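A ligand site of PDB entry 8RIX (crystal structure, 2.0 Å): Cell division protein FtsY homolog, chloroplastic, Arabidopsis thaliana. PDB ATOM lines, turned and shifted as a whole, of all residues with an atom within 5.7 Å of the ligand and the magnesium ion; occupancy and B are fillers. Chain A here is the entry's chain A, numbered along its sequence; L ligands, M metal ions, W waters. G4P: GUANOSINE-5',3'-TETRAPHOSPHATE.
O1A of the ligand lies within hydrogen-bond range of N of Thr 124 (3.1 Å).
The side-chain carboxylate (OD2) of Asp 267 is in hydrogen-bond range of a nitrogen (N2) of the ligand (2.4 Å).
N of Thr 125 lies within hydrogen-bond range of O1A of the ligand (2.7 Å).
OG1 of Thr 125 sits at hydrogen-bond distance from O1A of the ligand (3.1 Å).
The side-chain carboxylate (OE1) of Glu 293 lies within hydrogen-bond range of an oxygen (O2') of the ligand, 2.7 Å away.
The backbone NH of Lys 123 is in hydrogen-bond range of an oxygen (O3B) of the ligand (2.8 Å).
The side-chain amino group of Lys 123 lies within salt-bridge range of an oxygen (O3B) of the ligand (2.8 Å).
An oxygen (O6) of the ligand lies within hydrogen-bond range of the backbone NH of Lys 265, at 2.9 Å.
The side-chain amino group (NZ) of Lys 265 lies within hydrogen-bond range of an oxygen (O4') of the ligand (3.2 Å).
O1B of the ligand lies within hydrogen-bond range of N of Gly 120 (2.9 Å).
N of Gly 122 sits at hydrogen-bond distance from O3B of the ligand (3.1 Å).
O6 of the ligand lies within hydrogen-bond range of N of Gly 292 (3.3 Å).
N1 of the ligand sits close to O of Gly 292 (3.3 Å).
The side-chain amide nitrogen of Gln 156 lies within hydrogen-bond range of an oxygen (O2A) of the ligand (3.2 Å).
The backbone NH (N) of Val 291 is in hydrogen-bond range of an oxygen (O6) of the ligand (3.3 Å).
An oxygen (O3B) of the ligand sits at hydrogen-bond distance from the backbone NH (N) of Gly 121, at 3.5 Å.
OG1 of Thr 124 sits close to OD2 of Asp 200 (2.5 Å).
OG1 of Thr 125 sits at hydrogen-bond distance from O of Gly 122.
N of Glu 293 sits at hydrogen-bond distance from OD2 of Asp 297 (3.3 Å).
NZ of Lys 123 is in hydrogen-bond range of OD1 of Asn 119, at 2.8 Å.
The side-chain amino group of Lys 265 sits at hydrogen-bond distance from the backbone carbonyl oxygen of Gly 120.
The backbone NH (N) of Val 291 sits at hydrogen-bond distance from the backbone carbonyl oxygen (O) of Asp 297 (3.2 Å).
The backbone carbonyl oxygen of Gly 121 is in hydrogen-bond range of the side-chain hydroxyl of Thr 264.
The side-chain amino group (NZ) of Lys 129 sits at hydrogen-bond distance from the backbone carbonyl oxygen (O) of Asp 297 (2.7 Å).
The backbone carbonyl oxygen of Gly 290 lies close to an oxygen (O6) of the ligand, at 3.4 Å.
Val 118 touches the ligand.
CA of Asn 119 touches O1B of the ligand, 3.5 Å away.
Lys 129 touches the ligand.
Within 4 Å of the ligand: Val 118, Asn 119, Gly 120, Gly 121, Gly 122, Lys 123, Thr 124, Thr 125, Lys 129, Gln 156, Lys 265, Asp 267, Gly 290, Val 291, Gly 292 and Glu 293.
The nearest printed residue that does not touch the ligand is Thr 264 (4.01 Å).
Merely in contact with the magnesium ion: Asp 147, Gln 156 and Asp 200.
Four residues have an atom within 4 Å of the magnesium ion: Thr 124, Asp 147, Gln 156 and Asp 200.
Along chain A the residues within 4 Å of the magnesium ion span positions 124 to 200.
The nearest printed residue that does not touch the magnesium ion is Lys 123 (4.6 Å).
Water W4 binds the magnesium ion.
The magnesium ion is bound by water W3, 2.1 Å away.
Water W1 binds the magnesium ion, at 2.1 Å.
O2B of the ligand binds the magnesium ion.
The side-chain hydroxyl (OG1) of Thr 124 binds the magnesium ion, 2.1 Å away.
The magnesium ion is bound by water W6.
Water W3 bridges OD1 of Asp 200 (2.6 Å) and O of Thr 201 (3.1 Å).
Water W1 lies within hydrogen-bond range of OE1 of Gln 156 and O2A of the ligand.
Water W4 lies within hydrogen-bond range of an oxygen (O1B) of the ligand (2.7 Å), the side-chain amide oxygen (OD1) of Asn 119 (3.0 Å) and the side-chain carboxylate (OD2) of Asp 147 (3.2 Å).
Water W8 lies within hydrogen-bond range of NZ of Lys 129 (2.6 Å), N7 of the ligand (3.0 Å) and OG of Ser 126 (3.1 Å).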
ATOM      1  N   GLY A 117      11.909  22.141   6.847  1.00  0.00           N
ATOM      2  CA  GLY A 117      12.252  23.556   6.861  1.00  0.00           C
ATOM      3  C   GLY A 117      11.593  24.290   8.010  1.00  0.00           C
ATOM      4  O   GLY A 117      10.689  23.758   8.676  1.00  0.00           O
ATOM      5  N   VAL A 118      12.017  25.529   8.251  1.00  0.00           N
ATOM      6  CA  VAL A 118      11.475  26.285   9.377  1.00  0.00           C
ATOM      7  C   VAL A 118      10.056  26.723   9.052  1.00  0.00           C
ATOM      8  O   VAL A 118       9.702  26.940   7.886  1.00  0.00           O
ATOM      9  CB  VAL A 118      12.365  27.493   9.730  1.00  0.00           C
ATOM     10  CG1 VAL A 118      13.729  27.029  10.186  1.00  0.00           C
ATOM     11  CG2 VAL A 118      12.488  28.451   8.542  1.00  0.00           C
ATOM     12  N   ASN A 119       9.215  26.786  10.076  1.00  0.00           N
ATOM     13  CA  ASN A 119       7.849  27.230   9.857  1.00  0.00           C
ATOM     14  C   ASN A 119       7.852  28.651   9.298  1.00  0.00           C
ATOM     15  O   ASN A 119       8.770  29.428   9.524  1.00  0.00           O
ATOM     16  CB  ASN A 119       7.039  27.169  11.143  1.00  0.00           C
ATOM     17  CG  ASN A 119       6.531  25.768  11.441  1.00  0.00           C
ATOM     18  OD1 ASN A 119       6.611  24.865  10.581  1.00  0.00           O
ATOM     19  ND2 ASN A 119       5.980  25.579  12.624  1.00  0.00           N
ATOM     20  N   GLY A 120       6.791  28.968   8.556  1.00  0.00           N
ATOM     21  CA  GLY A 120       6.672  30.220   7.870  1.00  0.00           C
ATOM     22  C   GLY A 120       7.142  30.178   6.438  1.00  0.00           C
ATOM     23  O   GLY A 120       6.679  30.968   5.625  1.00  0.00           O
ATOM     24  N   GLY A 121       8.026  29.228   6.114  1.00  0.00           N
ATOM     25  CA  GLY A 121       8.725  29.289   4.849  1.00  0.00           C
ATOM     26  C   GLY A 121       7.913  28.802   3.668  1.00  0.00           C
ATOM     27  O   GLY A 121       8.189  29.204   2.529  1.00  0.00           O
ATOM     28  N   GLY A 122       6.937  27.923   3.906  1.00  0.00           N
ATOM     29  CA  GLY A 122       6.069  27.428   2.862  1.00  0.00           C
ATOM     30  C   GLY A 122       6.029  25.904   2.668  1.00  0.00           C
ATOM     31  O   GLY A 122       5.701  25.454   1.559  1.00  0.00           O
ATOM     32  N   LYS A 123       6.343  25.105   3.705  1.00  0.00           N
ATOM     33  CA  LYS A 123       6.331  23.644   3.542  1.00  0.00           C
ATOM     34  C   LYS A 123       4.948  23.152   3.118  1.00  0.00           C
ATOM     35  O   LYS A 123       4.796  22.483   2.096  1.00  0.00           O
ATOM     36  CB  LYS A 123       6.732  22.951   4.851  1.00  0.00           C
ATOM     37  CG  LYS A 123       8.168  23.211   5.305  1.00  0.00           C
ATOM     38  CD  LYS A 123       8.493  22.402   6.580  1.00  0.00           C
ATOM     39  CE  LYS A 123       7.583  22.816   7.748  1.00  0.00           C
ATOM     40  NZ  LYS A 123       7.717  24.264   8.073  1.00  0.00           N
ATOM     41  N   THR A 124       3.934  23.464   3.912  1.00  0.00           N
ATOM     42  CA  THR A 124       2.609  22.897   3.672  1.00  0.00           C
ATOM     43  C   THR A 124       2.056  23.334   2.325  1.00  0.00           C
ATOM     44  O   THR A 124       1.519  22.523   1.563  1.00  0.00           O
ATOM     45  CB  THR A 124       1.682  23.295   4.823  1.00  0.00           C
ATOM     46  OG1 THR A 124       2.287  22.877   6.060  1.00  0.00           O
ATOM     47  CG2 THR A 124       0.281  22.745   4.649  1.00  0.00           C
ATOM     48  N   THR A 125       2.200  24.615   1.987  1.00  0.00           N
ATOM     49  CA  THR A 125       1.685  25.046   0.691  1.00  0.00           C
ATOM     50  C   THR A 125       2.503  24.475  -0.461  1.00  0.00           C
ATOM     51  O   THR A 125       1.936  24.110  -1.494  1.00  0.00           O
ATOM     52  CB  THR A 125       1.657  26.574   0.603  1.00  0.00           C
ATOM     53  OG1 THR A 125       2.976  27.058   0.808  1.00  0.00           O
ATOM     54  CG2 THR A 125       0.760  27.179   1.684  1.00  0.00           C
ATOM     55  N   SER A 126       3.840  24.427  -0.311  1.00  0.00           N
ATOM     56  CA  SER A 126       4.658  23.797  -1.355  1.00  0.00           C
ATOM     57  C   SER A 126       4.253  22.339  -1.547  1.00  0.00           C
ATOM     58  O   SER A 126       4.178  21.845  -2.667  1.00  0.00           O
ATOM     59  CB  SER A 126       6.145  23.896  -1.014  1.00  0.00           C
ATOM     60  OG  SER A 126       6.634  25.258  -1.054  1.00  0.00           O
ATOM     61  N   LYS A 129       0.987  22.151  -3.557  1.00  0.00           N
ATOM     62  CA  LYS A 129       1.268  22.512  -4.940  1.00  0.00           C
ATOM     63  C   LYS A 129       2.008  21.391  -5.654  1.00  0.00           C
ATOM     64  O   LYS A 129       1.724  21.089  -6.818  1.00  0.00           O
ATOM     65  CB  LYS A 129       2.058  23.818  -5.013  1.00  0.00           C
ATOM     66  CG  LYS A 129       1.283  25.033  -4.472  1.00  0.00           C
ATOM     67  CD  LYS A 129       1.925  26.386  -4.805  1.00  0.00           C
ATOM     68  CE  LYS A 129       3.295  26.624  -4.148  1.00  0.00           C
ATOM     69  NZ  LYS A 129       3.829  28.070  -4.359  1.00  0.00           N
ATOM     70  N   ASP A 147       3.178  17.361  10.618  1.00  0.00           N
ATOM     71  CA  ASP A 147       3.297  18.502  11.531  1.00  0.00           C
ATOM     72  C   ASP A 147       2.221  18.325  12.592  1.00  0.00           C
ATOM     73  O   ASP A 147       1.046  18.625  12.369  1.00  0.00           O
ATOM     74  CB  ASP A 147       3.153  19.821  10.774  1.00  0.00           C
ATOM     75  CG  ASP A 147       3.293  21.031  11.677  1.00  0.00           C
ATOM     76  OD1 ASP A 147       3.622  20.844  12.874  1.00  0.00           O
ATOM     77  OD2 ASP A 147       3.127  22.182  11.178  1.00  0.00           O
ATOM     78  N   ALA A 153      -2.603  22.703  11.688  1.00  0.00           N
ATOM     79  CA  ALA A 153      -1.655  22.272  10.658  1.00  0.00           C
ATOM     80  C   ALA A 153      -2.216  21.119   9.841  1.00  0.00           C
ATOM     81  O   ALA A 153      -2.097  21.107   8.602  1.00  0.00           O
ATOM     82  CB  ALA A 153      -0.330  21.886  11.309  1.00  0.00           C
ATOM     83  N   GLN A 156      -5.138  22.528   7.810  1.00  0.00           N
ATOM     84  CA  GLN A 156      -4.619  23.232   6.639  1.00  0.00           C
ATOM     85  C   GLN A 156      -4.203  22.247   5.556  1.00  0.00           C
ATOM     86  O   GLN A 156      -4.595  22.391   4.386  1.00  0.00           O
ATOM     87  CB  GLN A 156      -3.459  24.124   7.034  1.00  0.00           C
ATOM     88  CG  GLN A 156      -2.544  24.455   5.861  1.00  0.00           C
ATOM     89  CD  GLN A 156      -1.351  25.270   6.291  1.00  0.00           C
ATOM     90  OE1 GLN A 156      -0.700  24.940   7.283  1.00  0.00           O
ATOM     91  NE2 GLN A 156      -1.022  26.316   5.521  1.00  0.00           N
ATOM     92  N   ASP A 200       4.392  16.151   5.176  1.00  0.00           N
ATOM     93  CA  ASP A 200       4.581  17.435   5.844  1.00  0.00           C
ATOM     94  C   ASP A 200       5.248  17.163   7.181  1.00  0.00           C
ATOM     95  O   ASP A 200       5.057  16.098   7.773  1.00  0.00           O
ATOM     96  CB  ASP A 200       3.242  18.145   6.042  1.00  0.00           C
ATOM     97  CG  ASP A 200       3.389  19.669   6.185  1.00  0.00           C
ATOM     98  OD1 ASP A 200       4.534  20.156   6.341  1.00  0.00           O
ATOM     99  OD2 ASP A 200       2.357  20.380   6.156  1.00  0.00           O
ATOM    100  N   THR A 201       6.076  18.101   7.634  1.00  0.00           N
ATOM    101  CA  THR A 201       6.785  17.972   8.899  1.00  0.00           C
ATOM    102  C   THR A 201       6.688  19.284   9.679  1.00  0.00           C
ATOM    103  O   THR A 201       6.326  20.334   9.128  1.00  0.00           O
ATOM    104  CB  THR A 201       8.264  17.611   8.714  1.00  0.00           C
ATOM    105  OG1 THR A 201       8.953  18.698   8.057  1.00  0.00           O
ATOM    106  CG2 THR A 201       8.461  16.282   7.925  1.00  0.00           C
ATOM    107  N   VAL A 236      12.628  23.593   2.342  1.00  0.00           N
ATOM    108  CA  VAL A 236      11.943  24.806   1.911  1.00  0.00           C
ATOM    109  C   VAL A 236      12.650  25.976   2.569  1.00  0.00           C
ATOM    110  O   VAL A 236      12.845  25.980   3.790  1.00  0.00           O
ATOM    111  CB  VAL A 236      10.456  24.777   2.296  1.00  0.00           C
ATOM    112  CG1 VAL A 236       9.807  26.135   2.024  1.00  0.00           C
ATOM    113  CG2 VAL A 236       9.756  23.652   1.570  1.00  0.00           C
ATOM    114  N   THR A 264      10.978  29.527  -1.998  1.00  0.00           N
ATOM    115  CA  THR A 264       9.612  30.017  -2.109  1.00  0.00           C
ATOM    116  C   THR A 264       9.583  31.539  -2.123  1.00  0.00           C
ATOM    117  O   THR A 264      10.578  32.218  -1.825  1.00  0.00           O
ATOM    118  CB  THR A 264       8.774  29.519  -0.941  1.00  0.00           C
ATOM    119  OG1 THR A 264       9.301  30.100   0.259  1.00  0.00           O
ATOM    120  CG2 THR A 264       8.828  27.929  -0.857  1.00  0.00           C
ATOM    121  N   LYS A 265       8.396  32.064  -2.439  1.00  0.00           N
ATOM    122  CA  LYS A 265       8.082  33.500  -2.344  1.00  0.00           C
ATOM    123  C   LYS A 265       8.953  34.313  -3.294  1.00  0.00           C
ATOM    124  O   LYS A 265       9.335  35.459  -3.001  1.00  0.00           O
ATOM    125  CB  LYS A 265       8.186  34.010  -0.911  1.00  0.00           C
ATOM    126  CG  LYS A 265       7.390  33.156   0.039  1.00  0.00           C
ATOM    127  CD  LYS A 265       7.389  33.682   1.452  1.00  0.00           C
ATOM    128  CE  LYS A 265       6.872  32.582   2.361  1.00  0.00           C
ATOM    129  NZ  LYS A 265       6.465  33.125   3.676  1.00  0.00           N
ATOM    130  N   LEU A 266       9.302  33.715  -4.426  1.00  0.00           N
ATOM    131  CA  LEU A 266      10.105  34.428  -5.397  1.00  0.00           C
ATOM    132  C   LEU A 266       9.244  35.177  -6.414  1.00  0.00           C
ATOM    133  O   LEU A 266       9.757  35.556  -7.477  1.00  0.00           O
ATOM    134  CB  LEU A 266      11.064  33.465  -6.098  1.00  0.00           C
ATOM    135  CG  LEU A 266      12.233  33.093  -5.168  1.00  0.00           C
ATOM    136  CD1 LEU A 266      13.242  32.220  -5.877  1.00  0.00           C
ATOM    137  CD2 LEU A 266      12.899  34.335  -4.592  1.00  0.00           C
ATOM    138  N   ASP A 267       7.961  35.413  -6.105  1.00  0.00           N
ATOM    139  CA  ASP A 267       7.031  36.007  -7.049  1.00  0.00           C
ATOM    140  C   ASP A 267       7.616  37.305  -7.588  1.00  0.00           C
ATOM    141  O   ASP A 267       7.840  38.248  -6.826  1.00  0.00           O
ATOM    142  CB  ASP A 267       5.671  36.300  -6.400  1.00  0.00           C
ATOM    143  CG  ASP A 267       5.345  35.410  -5.233  1.00  0.00           C
ATOM    144  OD1 ASP A 267       6.152  34.529  -4.862  1.00  0.00           O
ATOM    145  OD2 ASP A 267       4.254  35.588  -4.662  1.00  0.00           O
ATOM    146  N   GLY A 290       8.895  28.579  -5.649  1.00  0.00           N
ATOM    147  CA  GLY A 290       7.556  29.039  -5.349  1.00  0.00           C
ATOM    148  C   GLY A 290       7.453  30.461  -5.856  1.00  0.00           C
ATOM    149  O   GLY A 290       8.334  31.284  -5.614  1.00  0.00           O
ATOM    150  N   VAL A 291       6.381  30.744  -6.593  1.00  0.00           N
ATOM    151  CA  VAL A 291       6.267  32.027  -7.277  1.00  0.00           C
ATOM    152  C   VAL A 291       4.894  32.632  -7.026  1.00  0.00           C
ATOM    153  O   VAL A 291       4.403  33.420  -7.834  1.00  0.00           O
ATOM    154  CB  VAL A 291       6.537  31.892  -8.787  1.00  0.00           C
ATOM    155  CG1 VAL A 291       7.995  31.416  -9.069  1.00  0.00           C
ATOM    156  CG2 VAL A 291       5.522  30.981  -9.445  1.00  0.00           C
ATOM    157  N   GLY A 292       4.250  32.268  -5.924  1.00  0.00           N
ATOM    158  CA  GLY A 292       2.915  32.737  -5.645  1.00  0.00           C
ATOM    159  C   GLY A 292       2.155  31.765  -4.750  1.00  0.00           C
ATOM    160  O   GLY A 292       2.697  30.740  -4.317  1.00  0.00           O
ATOM    161  N   GLU A 293       0.900  32.112  -4.484  1.00  0.00           N
ATOM    162  CA  GLU A 293       0.073  31.338  -3.552  1.00  0.00           C
ATOM    163  C   GLU A 293      -0.970  30.456  -4.233  1.00  0.00           C
ATOM    164  O   GLU A 293      -1.627  29.667  -3.546  1.00  0.00           O
ATOM    165  CB  GLU A 293      -0.610  32.261  -2.545  1.00  0.00           C
ATOM    166  CG  GLU A 293       0.389  32.992  -1.680  1.00  0.00           C
ATOM    167  CD  GLU A 293      -0.220  33.899  -0.625  1.00  0.00           C
ATOM    168  OE1 GLU A 293      -0.642  33.382   0.441  1.00  0.00           O
ATOM    169  OE2 GLU A 293      -0.233  35.136  -0.849  1.00  0.00           O
ATOM    170  N   ASP A 297       1.401  27.655  -8.661  1.00  0.00           N
ATOM    171  CA  ASP A 297       2.577  28.509  -8.489  1.00  0.00           C
ATOM    172  C   ASP A 297       3.783  27.771  -7.901  1.00  0.00           C
ATOM    173  O   ASP A 297       4.422  28.240  -6.945  1.00  0.00           O
ATOM    174  CB  ASP A 297       2.191  29.716  -7.637  1.00  0.00           C
ATOM    175  CG  ASP A 297       1.299  30.698  -8.384  1.00  0.00           C
ATOM    176  OD1 ASP A 297       1.203  30.586  -9.624  1.00  0.00           O
ATOM    177  OD2 ASP A 297       0.691  31.586  -7.724  1.00  0.00           O
HETATM  178  PB  G4P L   1       5.000  26.349   6.691  1.00  0.00           P
HETATM  179  O1B G4P L   1       4.872  26.782   8.119  1.00  0.00           O
HETATM  180  O2B G4P L   1       4.154  25.129   6.340  1.00  0.00           O
HETATM  181  O3B G4P L   1       6.444  26.123   6.362  1.00  0.00           O
HETATM  182  O3A G4P L   1       4.474  27.521   5.727  1.00  0.00           O
HETATM  183  PA  G4P L   1       3.102  27.491   4.900  1.00  0.00           P
HETATM  184  O1A G4P L   1       3.042  26.442   3.818  1.00  0.00           O
HETATM  185  O2A G4P L   1       1.963  27.432   5.893  1.00  0.00           O
HETATM  186  O5' G4P L   1       3.177  28.957   4.100  1.00  0.00           O
HETATM  187  C5' G4P L   1       3.368  30.103   4.887  1.00  0.00           C
HETATM  188  C4' G4P L   1       2.880  31.268   4.066  1.00  0.00           C
HETATM  189  O4' G4P L   1       3.747  31.506   3.120  1.00  0.00           O
HETATM  190  C3' G4P L   1       1.419  30.897   3.357  1.00  0.00           C
HETATM  191  O3' G4P L   1       0.551  32.098   3.423  1.00  0.00           O
HETATM  192  C2' G4P L   1       1.654  30.614   2.167  1.00  0.00           C
HETATM  193  O2' G4P L   1       0.548  31.055   1.256  1.00  0.00           O
HETATM  194  C1' G4P L   1       2.906  31.549   1.881  1.00  0.00           C
HETATM  195  N9  G4P L   1       3.560  31.372   0.716  1.00  0.00           N
HETATM  196  C8  G4P L   1       4.105  30.128   0.720  1.00  0.00           C
HETATM  197  N7  G4P L   1       4.774  29.975  -0.478  1.00  0.00           N
HETATM  198  C5  G4P L   1       4.654  31.124  -1.177  1.00  0.00           C
HETATM  199  C6  G4P L   1       5.116  31.677  -2.550  1.00  0.00           C
HETATM  200  O6  G4P L   1       5.792  31.052  -3.321  1.00  0.00           O
HETATM  201  N1  G4P L   1       4.730  33.007  -2.936  1.00  0.00           N
HETATM  202  C2  G4P L   1       3.941  33.825  -2.060  1.00  0.00           C
HETATM  203  N2  G4P L   1       3.522  35.147  -2.396  1.00  0.00           N
HETATM  204  N3  G4P L   1       3.495  33.310  -0.790  1.00  0.00           N
HETATM  205  C4  G4P L   1       3.897  31.948  -0.404  1.00  0.00           C
HETATM  206  PC  G4P L   1      -0.116  32.536   4.896  1.00  0.00           P
HETATM  207  O1C G4P L   1       0.831  32.390   6.071  1.00  0.00           O
HETATM  208  O2C G4P L   1      -0.559  33.980   4.782  1.00  0.00           O
HETATM  209  O3C G4P L   1      -1.392  31.507   5.207  1.00  0.00           O
HETATM  210  PD  G4P L   1      -2.517  31.199   4.043  1.00  0.00           P
HETATM  211  O1D G4P L   1      -2.389  29.771   3.530  1.00  0.00           O
HETATM  212  O2D G4P L   1      -3.906  31.413   4.617  1.00  0.00           O
HETATM  213  O3D G4P L   1      -2.243  32.182   2.912  1.00  0.00           O
HETATM  214 MG    MG M   1       3.090  23.927   7.716  1.00  0.00          MG
HETATM  215  O   HOH W   1       1.677  25.476   7.522  1.00  0.00           O
HETATM  216  O   HOH W   2       2.837  28.900   9.001  1.00  0.00           O
HETATM  217  O   HOH W   3       4.410  22.297   7.746  1.00  0.00           O
HETATM  218  O   HOH W   4       3.860  24.677   9.378  1.00  0.00           O
HETATM  219  O   HOH W   5       0.827  29.296   7.602  1.00  0.00           O
HETATM  220  O   HOH W   6       1.643  22.721   9.080  1.00  0.00           O
HETATM  221  O   HOH W   7       2.633  31.334   8.330  1.00  0.00           O
HETATM  222  O   HOH W   8       5.613  27.804  -2.443  1.00  0.00           O
